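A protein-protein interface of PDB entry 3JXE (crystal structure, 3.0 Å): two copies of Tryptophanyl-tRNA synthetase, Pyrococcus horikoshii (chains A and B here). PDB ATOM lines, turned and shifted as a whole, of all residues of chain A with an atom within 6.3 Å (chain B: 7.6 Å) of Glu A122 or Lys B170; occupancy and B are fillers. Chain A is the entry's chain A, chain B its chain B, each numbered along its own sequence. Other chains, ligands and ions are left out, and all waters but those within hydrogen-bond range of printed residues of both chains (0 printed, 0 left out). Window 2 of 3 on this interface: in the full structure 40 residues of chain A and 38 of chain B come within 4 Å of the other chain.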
ATOM      1  N   LYS A 117     -12.553 -23.890 -13.797  1.00  0.00           N
ATOM      2  CA  LYS A 117     -12.712 -25.330 -13.978  1.00  0.00           C
ATOM      3  C   LYS A 117     -12.296 -25.833 -15.353  1.00  0.00           C
ATOM      4  O   LYS A 117     -11.898 -26.988 -15.495  1.00  0.00           O
ATOM      5  CB  LYS A 117     -14.133 -25.771 -13.624  1.00  0.00           C
ATOM      6  CG  LYS A 117     -14.480 -25.585 -12.151  1.00  0.00           C
ATOM      7  CD  LYS A 117     -13.367 -26.100 -11.244  1.00  0.00           C
ATOM      8  CE  LYS A 117     -13.691 -25.872  -9.777  1.00  0.00           C
ATOM      9  NZ  LYS A 117     -12.471 -25.980  -8.931  1.00  0.00           N
ATOM     10  N   PHE A 118     -12.375 -24.968 -16.360  1.00  0.00           N
ATOM     11  CA  PHE A 118     -11.794 -25.287 -17.654  1.00  0.00           C
ATOM     12  C   PHE A 118     -10.272 -25.323 -17.550  1.00  0.00           C
ATOM     13  O   PHE A 118      -9.649 -26.305 -17.951  1.00  0.00           O
ATOM     14  CB  PHE A 118     -12.240 -24.297 -18.731  1.00  0.00           C
ATOM     15  CG  PHE A 118     -11.498 -24.443 -20.035  1.00  0.00           C
ATOM     16  CD1 PHE A 118     -11.439 -25.668 -20.695  1.00  0.00           C
ATOM     17  CD2 PHE A 118     -10.861 -23.352 -20.607  1.00  0.00           C
ATOM     18  CE1 PHE A 118     -10.758 -25.799 -21.904  1.00  0.00           C
ATOM     19  CE2 PHE A 118     -10.175 -23.473 -21.817  1.00  0.00           C
ATOM     20  CZ  PHE A 118     -10.125 -24.697 -22.465  1.00  0.00           C
ATOM     21  N   LEU A 119      -9.691 -24.259 -16.999  1.00  0.00           N
ATOM     22  CA  LEU A 119      -8.239 -24.119 -16.876  1.00  0.00           C
ATOM     23  C   LEU A 119      -7.594 -25.200 -16.003  1.00  0.00           C
ATOM     24  O   LEU A 119      -6.539 -25.732 -16.350  1.00  0.00           O
ATOM     25  CB  LEU A 119      -7.876 -22.730 -16.335  1.00  0.00           C
ATOM     26  CG  LEU A 119      -8.136 -21.490 -17.197  1.00  0.00           C
ATOM     27  CD1 LEU A 119      -8.178 -20.247 -16.328  1.00  0.00           C
ATOM     28  CD2 LEU A 119      -7.100 -21.337 -18.305  1.00  0.00           C
ATOM     29  N   PHE A 120      -8.241 -25.524 -14.885  1.00  0.00           N
ATOM     30  CA  PHE A 120      -7.666 -26.416 -13.875  1.00  0.00           C
ATOM     31  C   PHE A 120      -7.918 -27.911 -14.098  1.00  0.00           C
ATOM     32  O   PHE A 120      -7.370 -28.742 -13.370  1.00  0.00           O
ATOM     33  CB  PHE A 120      -8.132 -26.006 -12.474  1.00  0.00           C
ATOM     34  CG  PHE A 120      -7.347 -24.869 -11.882  1.00  0.00           C
ATOM     35  CD1 PHE A 120      -7.654 -23.550 -12.199  1.00  0.00           C
ATOM     36  CD2 PHE A 120      -6.301 -25.118 -11.004  1.00  0.00           C
ATOM     37  CE1 PHE A 120      -6.929 -22.498 -11.652  1.00  0.00           C
ATOM     38  CE2 PHE A 120      -5.567 -24.073 -10.457  1.00  0.00           C
ATOM     39  CZ  PHE A 120      -5.885 -22.761 -10.781  1.00  0.00           C
ATOM     40  N   LYS A 121      -8.737 -28.255 -15.089  1.00  0.00           N
ATOM     41  CA  LYS A 121      -9.009 -29.660 -15.399  1.00  0.00           C
ATOM     42  C   LYS A 121      -8.851 -29.987 -16.878  1.00  0.00           C
ATOM     43  O   LYS A 121      -9.414 -29.310 -17.738  1.00  0.00           O
ATOM     44  CB  LYS A 121     -10.383 -30.090 -14.873  1.00  0.00           C
ATOM     45  CG  LYS A 121     -10.310 -30.682 -13.463  1.00  0.00           C
ATOM     46  CD  LYS A 121     -11.676 -30.681 -12.774  1.00  0.00           C
ATOM     47  CE  LYS A 121     -11.541 -31.272 -11.366  1.00  0.00           C
ATOM     48  NZ  LYS A 121     -12.814 -31.121 -10.577  1.00  0.00           N
ATOM     49  N   GLU A 122      -8.078 -31.031 -17.159  1.00  0.00           N
ATOM     50  CA  GLU A 122      -7.732 -31.395 -18.532  1.00  0.00           C
ATOM     51  C   GLU A 122      -8.854 -32.062 -19.323  1.00  0.00           C
ATOM     52  O   GLU A 122      -8.969 -31.842 -20.528  1.00  0.00           O
ATOM     53  CB  GLU A 122      -6.474 -32.265 -18.566  1.00  0.00           C
ATOM     54  CG  GLU A 122      -5.198 -31.492 -18.877  1.00  0.00           C
ATOM     55  CD  GLU A 122      -5.084 -31.074 -20.345  1.00  0.00           C
ATOM     56  OE1 GLU A 122      -3.935 -30.885 -20.812  1.00  0.00           O
ATOM     57  OE2 GLU A 122      -6.128 -30.936 -21.034  1.00  0.00           O
ATOM     58  N   ASN A 123      -9.664 -32.874 -18.645  1.00  0.00           N
ATOM     59  CA  ASN A 123     -10.781 -33.580 -19.280  1.00  0.00           C
ATOM     60  C   ASN A 123     -11.831 -32.609 -19.813  1.00  0.00           C
ATOM     61  O   ASN A 123     -12.377 -32.808 -20.901  1.00  0.00           O
ATOM     62  CB  ASN A 123     -11.463 -34.547 -18.299  1.00  0.00           C
ATOM     63  CG  ASN A 123     -10.699 -34.708 -16.995  1.00  0.00           C
ATOM     64  OD1 ASN A 123     -11.084 -34.145 -15.967  1.00  0.00           O
ATOM     65  ND2 ASN A 123      -9.606 -35.470 -17.033  1.00  0.00           N
ATOM     66  N   LEU A 124     -12.097 -31.561 -19.035  1.00  0.00           N
ATOM     67  CA  LEU A 124     -13.177 -30.618 -19.314  1.00  0.00           C
ATOM     68  C   LEU A 124     -12.820 -29.601 -20.389  1.00  0.00           C
ATOM     69  O   LEU A 124     -11.729 -29.028 -20.380  1.00  0.00           O
ATOM     70  CB  LEU A 124     -13.589 -29.892 -18.030  1.00  0.00           C
ATOM     71  CG  LEU A 124     -14.619 -30.517 -17.080  1.00  0.00           C
ATOM     72  CD1 LEU A 124     -14.253 -31.925 -16.616  1.00  0.00           C
ATOM     73  CD2 LEU A 124     -14.816 -29.609 -15.883  1.00  0.00           C
ATOM     74  N   THR A 125     -13.749 -29.395 -21.318  1.00  0.00           N
ATOM     75  CA  THR A 125     -13.637 -28.340 -22.319  1.00  0.00           C
ATOM     76  C   THR A 125     -14.375 -27.100 -21.827  1.00  0.00           C
ATOM     77  O   THR A 125     -15.252 -27.198 -20.965  1.00  0.00           O
ATOM     78  CB  THR A 125     -14.227 -28.767 -23.676  1.00  0.00           C
ATOM     79  OG1 THR A 125     -15.598 -29.148 -23.505  1.00  0.00           O
ATOM     80  CG2 THR A 125     -13.438 -29.926 -24.273  1.00  0.00           C
ATOM     81  N   PHE A 126     -14.024 -25.940 -22.382  1.00  0.00           N
ATOM     82  CA  PHE A 126     -14.630 -24.669 -21.977  1.00  0.00           C
ATOM     83  C   PHE A 126     -16.130 -24.686 -22.239  1.00  0.00           C
ATOM     84  O   PHE A 126     -16.905 -24.056 -21.521  1.00  0.00           O
ATOM     85  CB  PHE A 126     -13.964 -23.496 -22.711  1.00  0.00           C
ATOM     86  CG  PHE A 126     -14.140 -22.157 -22.029  1.00  0.00           C
ATOM     87  CD1 PHE A 126     -13.987 -20.977 -22.751  1.00  0.00           C
ATOM     88  CD2 PHE A 126     -14.453 -22.072 -20.672  1.00  0.00           C
ATOM     89  CE1 PHE A 126     -14.137 -19.735 -22.134  1.00  0.00           C
ATOM     90  CE2 PHE A 126     -14.612 -20.837 -20.048  1.00  0.00           C
ATOM     91  CZ  PHE A 126     -14.452 -19.668 -20.781  1.00  0.00           C
ATOM     92  N   LYS A 188      -0.554 -23.665 -15.700  1.00  0.00           N
ATOM     93  CA  LYS A 188      -0.908 -22.864 -16.866  1.00  0.00           C
ATOM     94  C   LYS A 188      -0.978 -21.395 -16.462  1.00  0.00           C
ATOM     95  O   LYS A 188      -1.315 -21.080 -15.316  1.00  0.00           O
ATOM     96  CB  LYS A 188      -2.240 -23.326 -17.469  1.00  0.00           C
ATOM     97  CG  LYS A 188      -2.358 -24.830 -17.748  1.00  0.00           C
ATOM     98  CD  LYS A 188      -1.107 -25.409 -18.402  1.00  0.00           C
ATOM     99  CE  LYS A 188      -1.253 -26.894 -18.662  1.00  0.00           C
ATOM    100  NZ  LYS A 188      -2.028 -27.163 -19.905  1.00  0.00           N
ATOM    101  N   ILE A 189      -0.657 -20.501 -17.395  1.00  0.00           N
ATOM    102  CA  ILE A 189      -0.670 -19.063 -17.101  1.00  0.00           C
ATOM    103  C   ILE A 189      -2.047 -18.593 -16.625  1.00  0.00           C
ATOM    104  O   ILE A 189      -2.145 -17.692 -15.787  1.00  0.00           O
ATOM    105  CB  ILE A 189      -0.134 -18.192 -18.275  1.00  0.00           C
ATOM    106  CG1 ILE A 189      -0.950 -18.406 -19.555  1.00  0.00           C
ATOM    107  CG2 ILE A 189       1.348 -18.478 -18.509  1.00  0.00           C
ATOM    108  CD1 ILE A 189      -0.635 -17.420 -20.670  1.00  0.00           C
ATOM    109  N   GLY A 190      -3.098 -19.227 -17.145  1.00  0.00           N
ATOM    110  CA  GLY A 190      -4.467 -18.972 -16.703  1.00  0.00           C
ATOM    111  C   GLY A 190      -4.694 -19.409 -15.269  1.00  0.00           C
ATOM    112  O   GLY A 190      -5.440 -18.765 -14.528  1.00  0.00           O
ATOM    113  N   ALA B 165      -9.210 -15.235 -24.279  1.00  0.00           N
ATOM    114  CA  ALA B 165      -7.842 -15.607 -23.909  1.00  0.00           C
ATOM    115  C   ALA B 165      -7.757 -16.942 -23.170  1.00  0.00           C
ATOM    116  O   ALA B 165      -6.727 -17.616 -23.217  1.00  0.00           O
ATOM    117  CB  ALA B 165      -7.204 -14.509 -23.074  1.00  0.00           C
ATOM    118  N   ILE B 166      -8.842 -17.313 -22.493  1.00  0.00           N
ATOM    119  CA  ILE B 166      -8.884 -18.521 -21.662  1.00  0.00           C
ATOM    120  C   ILE B 166      -8.384 -19.798 -22.375  1.00  0.00           C
ATOM    121  O   ILE B 166      -7.534 -20.501 -21.824  1.00  0.00           O
ATOM    122  CB  ILE B 166     -10.286 -18.727 -20.997  1.00  0.00           C
ATOM    123  CG1 ILE B 166     -10.626 -17.567 -20.049  1.00  0.00           C
ATOM    124  CG2 ILE B 166     -10.367 -20.059 -20.255  1.00  0.00           C
ATOM    125  CD1 ILE B 166      -9.673 -17.393 -18.866  1.00  0.00           C
ATOM    126  N   PRO B 167      -8.900 -20.102 -23.588  1.00  0.00           N
ATOM    127  CA  PRO B 167      -8.400 -21.273 -24.317  1.00  0.00           C
ATOM    128  C   PRO B 167      -6.869 -21.398 -24.374  1.00  0.00           C
ATOM    129  O   PRO B 167      -6.336 -22.455 -24.030  1.00  0.00           O
ATOM    130  CB  PRO B 167      -8.985 -21.082 -25.717  1.00  0.00           C
ATOM    131  CG  PRO B 167     -10.267 -20.387 -25.463  1.00  0.00           C
ATOM    132  CD  PRO B 167      -9.980 -19.430 -24.339  1.00  0.00           C
ATOM    133  N   ILE B 168      -6.174 -20.339 -24.787  1.00  0.00           N
ATOM    134  CA  ILE B 168      -4.708 -20.381 -24.880  1.00  0.00           C
ATOM    135  C   ILE B 168      -4.015 -20.187 -23.520  1.00  0.00           C
ATOM    136  O   ILE B 168      -2.848 -20.544 -23.352  1.00  0.00           O
ATOM    137  CB  ILE B 168      -4.147 -19.402 -25.961  1.00  0.00           C
ATOM    138  CG1 ILE B 168      -2.735 -19.834 -26.385  1.00  0.00           C
ATOM    139  CG2 ILE B 168      -4.188 -17.947 -25.475  1.00  0.00           C
ATOM    140  CD1 ILE B 168      -2.263 -19.274 -27.710  1.00  0.00           C
ATOM    141  N   ALA B 169      -4.742 -19.637 -22.551  1.00  0.00           N
ATOM    142  CA  ALA B 169      -4.223 -19.493 -21.193  1.00  0.00           C
ATOM    143  C   ALA B 169      -4.132 -20.851 -20.491  1.00  0.00           C
ATOM    144  O   ALA B 169      -3.501 -20.972 -19.439  1.00  0.00           O
ATOM    145  CB  ALA B 169      -5.081 -18.530 -20.394  1.00  0.00           C
ATOM    146  N   LYS B 170      -4.772 -21.858 -21.083  1.00  0.00           N
ATOM    147  CA  LYS B 170      -4.691 -23.240 -20.617  1.00  0.00           C
ATOM    148  C   LYS B 170      -3.621 -24.002 -21.397  1.00  0.00           C
ATOM    149  O   LYS B 170      -3.072 -24.984 -20.906  1.00  0.00           O
ATOM    150  CB  LYS B 170      -6.047 -23.934 -20.768  1.00  0.00           C
ATOM    151  CG  LYS B 170      -6.158 -25.272 -20.052  1.00  0.00           C
ATOM    152  CD  LYS B 170      -7.451 -25.984 -20.402  1.00  0.00           C
ATOM    153  CE  LYS B 170      -7.443 -27.419 -19.908  1.00  0.00           C
ATOM    154  NZ  LYS B 170      -8.752 -28.080 -20.133  1.00  0.00           N
ATOM    155  N   LYS B 171      -3.337 -23.548 -22.615  1.00  0.00           N
ATOM    156  CA  LYS B 171      -2.310 -24.166 -23.451  1.00  0.00           C
ATOM    157  C   LYS B 171      -0.913 -23.735 -23.018  1.00  0.00           C
ATOM    158  O   LYS B 171      -0.054 -24.577 -22.749  1.00  0.00           O
ATOM    159  CB  LYS B 171      -2.535 -23.835 -24.928  1.00  0.00           C
ATOM    160  CG  LYS B 171      -3.736 -24.529 -25.552  1.00  0.00           C
ATOM    161  CD  LYS B 171      -3.423 -25.969 -25.927  1.00  0.00           C
ATOM    162  CE  LYS B 171      -4.642 -26.671 -26.494  1.00  0.00           C
ATOM    163  NZ  LYS B 171      -4.256 -27.941 -27.162  1.00  0.00           N
ATOM    164  N   ILE B 172      -0.696 -22.423 -22.948  1.00  0.00           N
ATOM    165  CA  ILE B 172       0.599 -21.877 -22.553  1.00  0.00           C
ATOM    166  C   ILE B 172       0.847 -22.158 -21.076  1.00  0.00           C
ATOM    167  O   ILE B 172       0.243 -21.537 -20.197  1.00  0.00           O
ATOM    168  CB  ILE B 172       0.722 -20.355 -22.846  1.00  0.00           C
ATOM    169  CG1 ILE B 172       0.452 -20.065 -24.324  1.00  0.00           C
ATOM    170  CG2 ILE B 172       2.105 -19.847 -22.448  1.00  0.00           C
ATOM    171  CD1 ILE B 172       0.253 -18.598 -24.643  1.00  0.00           C
ATOM    172  N   ASN B 173       1.726 -23.119 -20.818  1.00  0.00           N
ATOM    173  CA  ASN B 173       2.139 -23.420 -19.458  1.00  0.00           C
ATOM    174  C   ASN B 173       3.178 -22.403 -18.997  1.00  0.00           C
ATOM    175  O   ASN B 173       3.725 -21.646 -19.803  1.00  0.00           O
ATOM    176  CB  ASN B 173       2.635 -24.871 -19.335  1.00  0.00           C
ATOM    177  CG  ASN B 173       4.150 -24.990 -19.327  1.00  0.00           C
ATOM    178  OD1 ASN B 173       4.730 -25.454 -18.349  1.00  0.00           O
ATOM    179  ND2 ASN B 173       4.793 -24.581 -20.413  1.00  0.00           N
ATOM    180  N   MET B 176       6.883 -22.237 -20.354  1.00  0.00           N
ATOM    181  CA  MET B 176       6.917 -21.572 -21.656  1.00  0.00           C
ATOM    182  C   MET B 176       6.962 -20.055 -21.532  1.00  0.00           C
ATOM    183  O   MET B 176       7.706 -19.391 -22.257  1.00  0.00           O
ATOM    184  CB  MET B 176       5.701 -21.974 -22.493  1.00  0.00           C
ATOM    185  CG  MET B 176       5.888 -23.246 -23.282  1.00  0.00           C
ATOM    186  SD  MET B 176       4.484 -23.607 -24.346  1.00  0.00           S
ATOM    187  CE  MET B 176       3.491 -24.640 -23.264  1.00  0.00           C
ATOM    188  N   PHE B 193      -0.015 -13.675 -17.058  1.00  0.00           N
ATOM    189  CA  PHE B 193      -1.232 -13.986 -17.797  1.00  0.00           C
ATOM    190  C   PHE B 193      -1.326 -13.225 -19.111  1.00  0.00           C
ATOM    191  O   PHE B 193      -1.874 -13.736 -20.089  1.00  0.00           O
ATOM    192  CB  PHE B 193      -2.461 -13.684 -16.946  1.00  0.00           C
ATOM    193  CG  PHE B 193      -3.766 -13.989 -17.630  1.00  0.00           C
ATOM    194  CD1 PHE B 193      -4.575 -12.962 -18.100  1.00  0.00           C
ATOM    195  CD2 PHE B 193      -4.184 -15.304 -17.809  1.00  0.00           C
ATOM    196  CE1 PHE B 193      -5.780 -13.237 -18.734  1.00  0.00           C
ATOM    197  CE2 PHE B 193      -5.388 -15.589 -18.441  1.00  0.00           C
ATOM    198  CZ  PHE B 193      -6.187 -14.553 -18.907  1.00  0.00           C
ATOM    199  N   ALA B 196      -1.582 -14.197 -23.036  1.00  0.00           N
ATOM    200  CA  ALA B 196      -2.854 -14.759 -23.491  1.00  0.00           C
ATOM    201  C   ALA B 196      -3.791 -13.674 -24.028  1.00  0.00           C
ATOM    202  O   ALA B 196      -4.517 -13.898 -24.998  1.00  0.00           O
ATOM    203  CB  ALA B 196      -3.525 -15.541 -22.371  1.00  0.00           C
ATOM    204  N   PHE B 227      -0.044 -23.115 -30.765  1.00  0.00           N
ATOM    205  CA  PHE B 227      -1.322 -23.661 -30.306  1.00  0.00           C
ATOM    206  C   PHE B 227      -2.526 -23.274 -31.163  1.00  0.00           C
ATOM    207  O   PHE B 227      -3.645 -23.702 -30.878  1.00  0.00           O
ATOM    208  CB  PHE B 227      -1.572 -23.271 -28.846  1.00  0.00           C
ATOM    209  CG  PHE B 227      -0.484 -23.704 -27.910  1.00  0.00           C
ATOM    210  CD1 PHE B 227       0.366 -22.767 -27.333  1.00  0.00           C
ATOM    211  CD2 PHE B 227      -0.301 -25.049 -27.608  1.00  0.00           C
ATOM    212  CE1 PHE B 227       1.377 -23.164 -26.464  1.00  0.00           C
ATOM    213  CE2 PHE B 227       0.707 -25.456 -26.741  1.00  0.00           C
ATOM    214  CZ  PHE B 227       1.546 -24.514 -26.169  1.00  0.00           C
ATOM    215  N   LEU B 231      -6.441 -25.063 -31.234  1.00  0.00           N
ATOM    216  CA  LEU B 231      -7.545 -24.228 -30.763  1.00  0.00           C
ATOM    217  C   LEU B 231      -8.576 -23.987 -31.867  1.00  0.00           C
ATOM    218  O   LEU B 231      -9.618 -23.371 -31.628  1.00  0.00           O
ATOM    219  CB  LEU B 231      -7.024 -22.895 -30.212  1.00  0.00           C
ATOM    220  CG  LEU B 231      -6.077 -22.926 -29.007  1.00  0.00           C
ATOM    221  CD1 LEU B 231      -5.424 -21.570 -28.816  1.00  0.00           C
ATOM    222  CD2 LEU B 231      -6.775 -23.378 -27.731  1.00  0.00           C
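The side-chain amide nitrogen of Asn B173 sits close to the backbone NH of Met B176, 3.1 Å away.
Among the printed residues, merely in contact across the chains: Lys A188 with Ala B169 (3.3 Å), Phe A118 with Ile B166 (3.3 Å), Ile A189 with Ala B169 (3.5 Å), Leu A119 with Ile B166 (3.6 Å), Leu A119 with Lys B170 (3.7 Å), Leu A119 with Ala B169 (3.7 Å), Ile A189 with Phe B193 (3.7 Å), Lys A188 with Ile B172 (3.8 Å), Phe A118 with Pro B167 (3.8 Å), Gly A190 with Phe B193 (3.8 Å), Ile A189 with Ala B196 (3.8 Å) and Lys A188 with Asn B173 (3.9 Å).
The side-chain amino group (NZ) of Lys B170 lies within hydrogen-bond range of the backbone carbonyl oxygen (O) of Lys A121 (2.8 Å). The backbone carbonyl oxygen of Leu A124 sits at hydrogen-bond distance from the side-chain amino group of Lys B170, 3.1 Å away. The side-chain amino group (NZ) of Lys A188 sits at hydrogen-bond distance from the backbone carbonyl oxygen (O) of Lys B170, 2.6 Å away. The backbone NH (N) of Gly A190 sits at hydrogen-bond distance from the backbone carbonyl oxygen (O) of Ala B169 (2.9 Å). N of Ile A189 sits at hydrogen-bond distance from O of Ile B172. NZ of Lys B170 lies within salt-bridge range of OE2 of Glu A122, at 3.98 Å. O of Phe A118 lies within hydrogen-bond range of NZ of Lys B170, 3.0 Å away.
Printed residues of chain B within 4 Å of Leu A119: Ile B166 (3.6 Å), Ala B169 (3.7 Å) and Lys B170 (3.7 Å). Of the printed residues of chain B, Glu A122 touches Lys B170 (3.8 Å). Of the printed residues of chain B, Lys A188 touches Ala B169 (3.3 Å), Lys B170 (2.6 Å), Ile B172 (3.8 Å) and Asn B173 (3.9 Å). Lys B170 touches just these residues of chain A: Phe A118, Leu A119, Lys A121, Glu A122, Leu A124 and Lys A188.
Hydrophobic or aromatic side chains of chain B within 4 Å of the printed part of chain A: Ile B166, Ala B169, Ile B172, Phe B193 and Ala B196. Printed residues of chain A that touch a printed residue of chain B: Phe A118, Leu A119, Lys A121, Glu A122, Leu A124, Lys A188, Ile A189 and Gly A190. Along chain A the printed residues that touch a printed residue of chain B span positions 118 to 190.
No position is printed for both chains.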
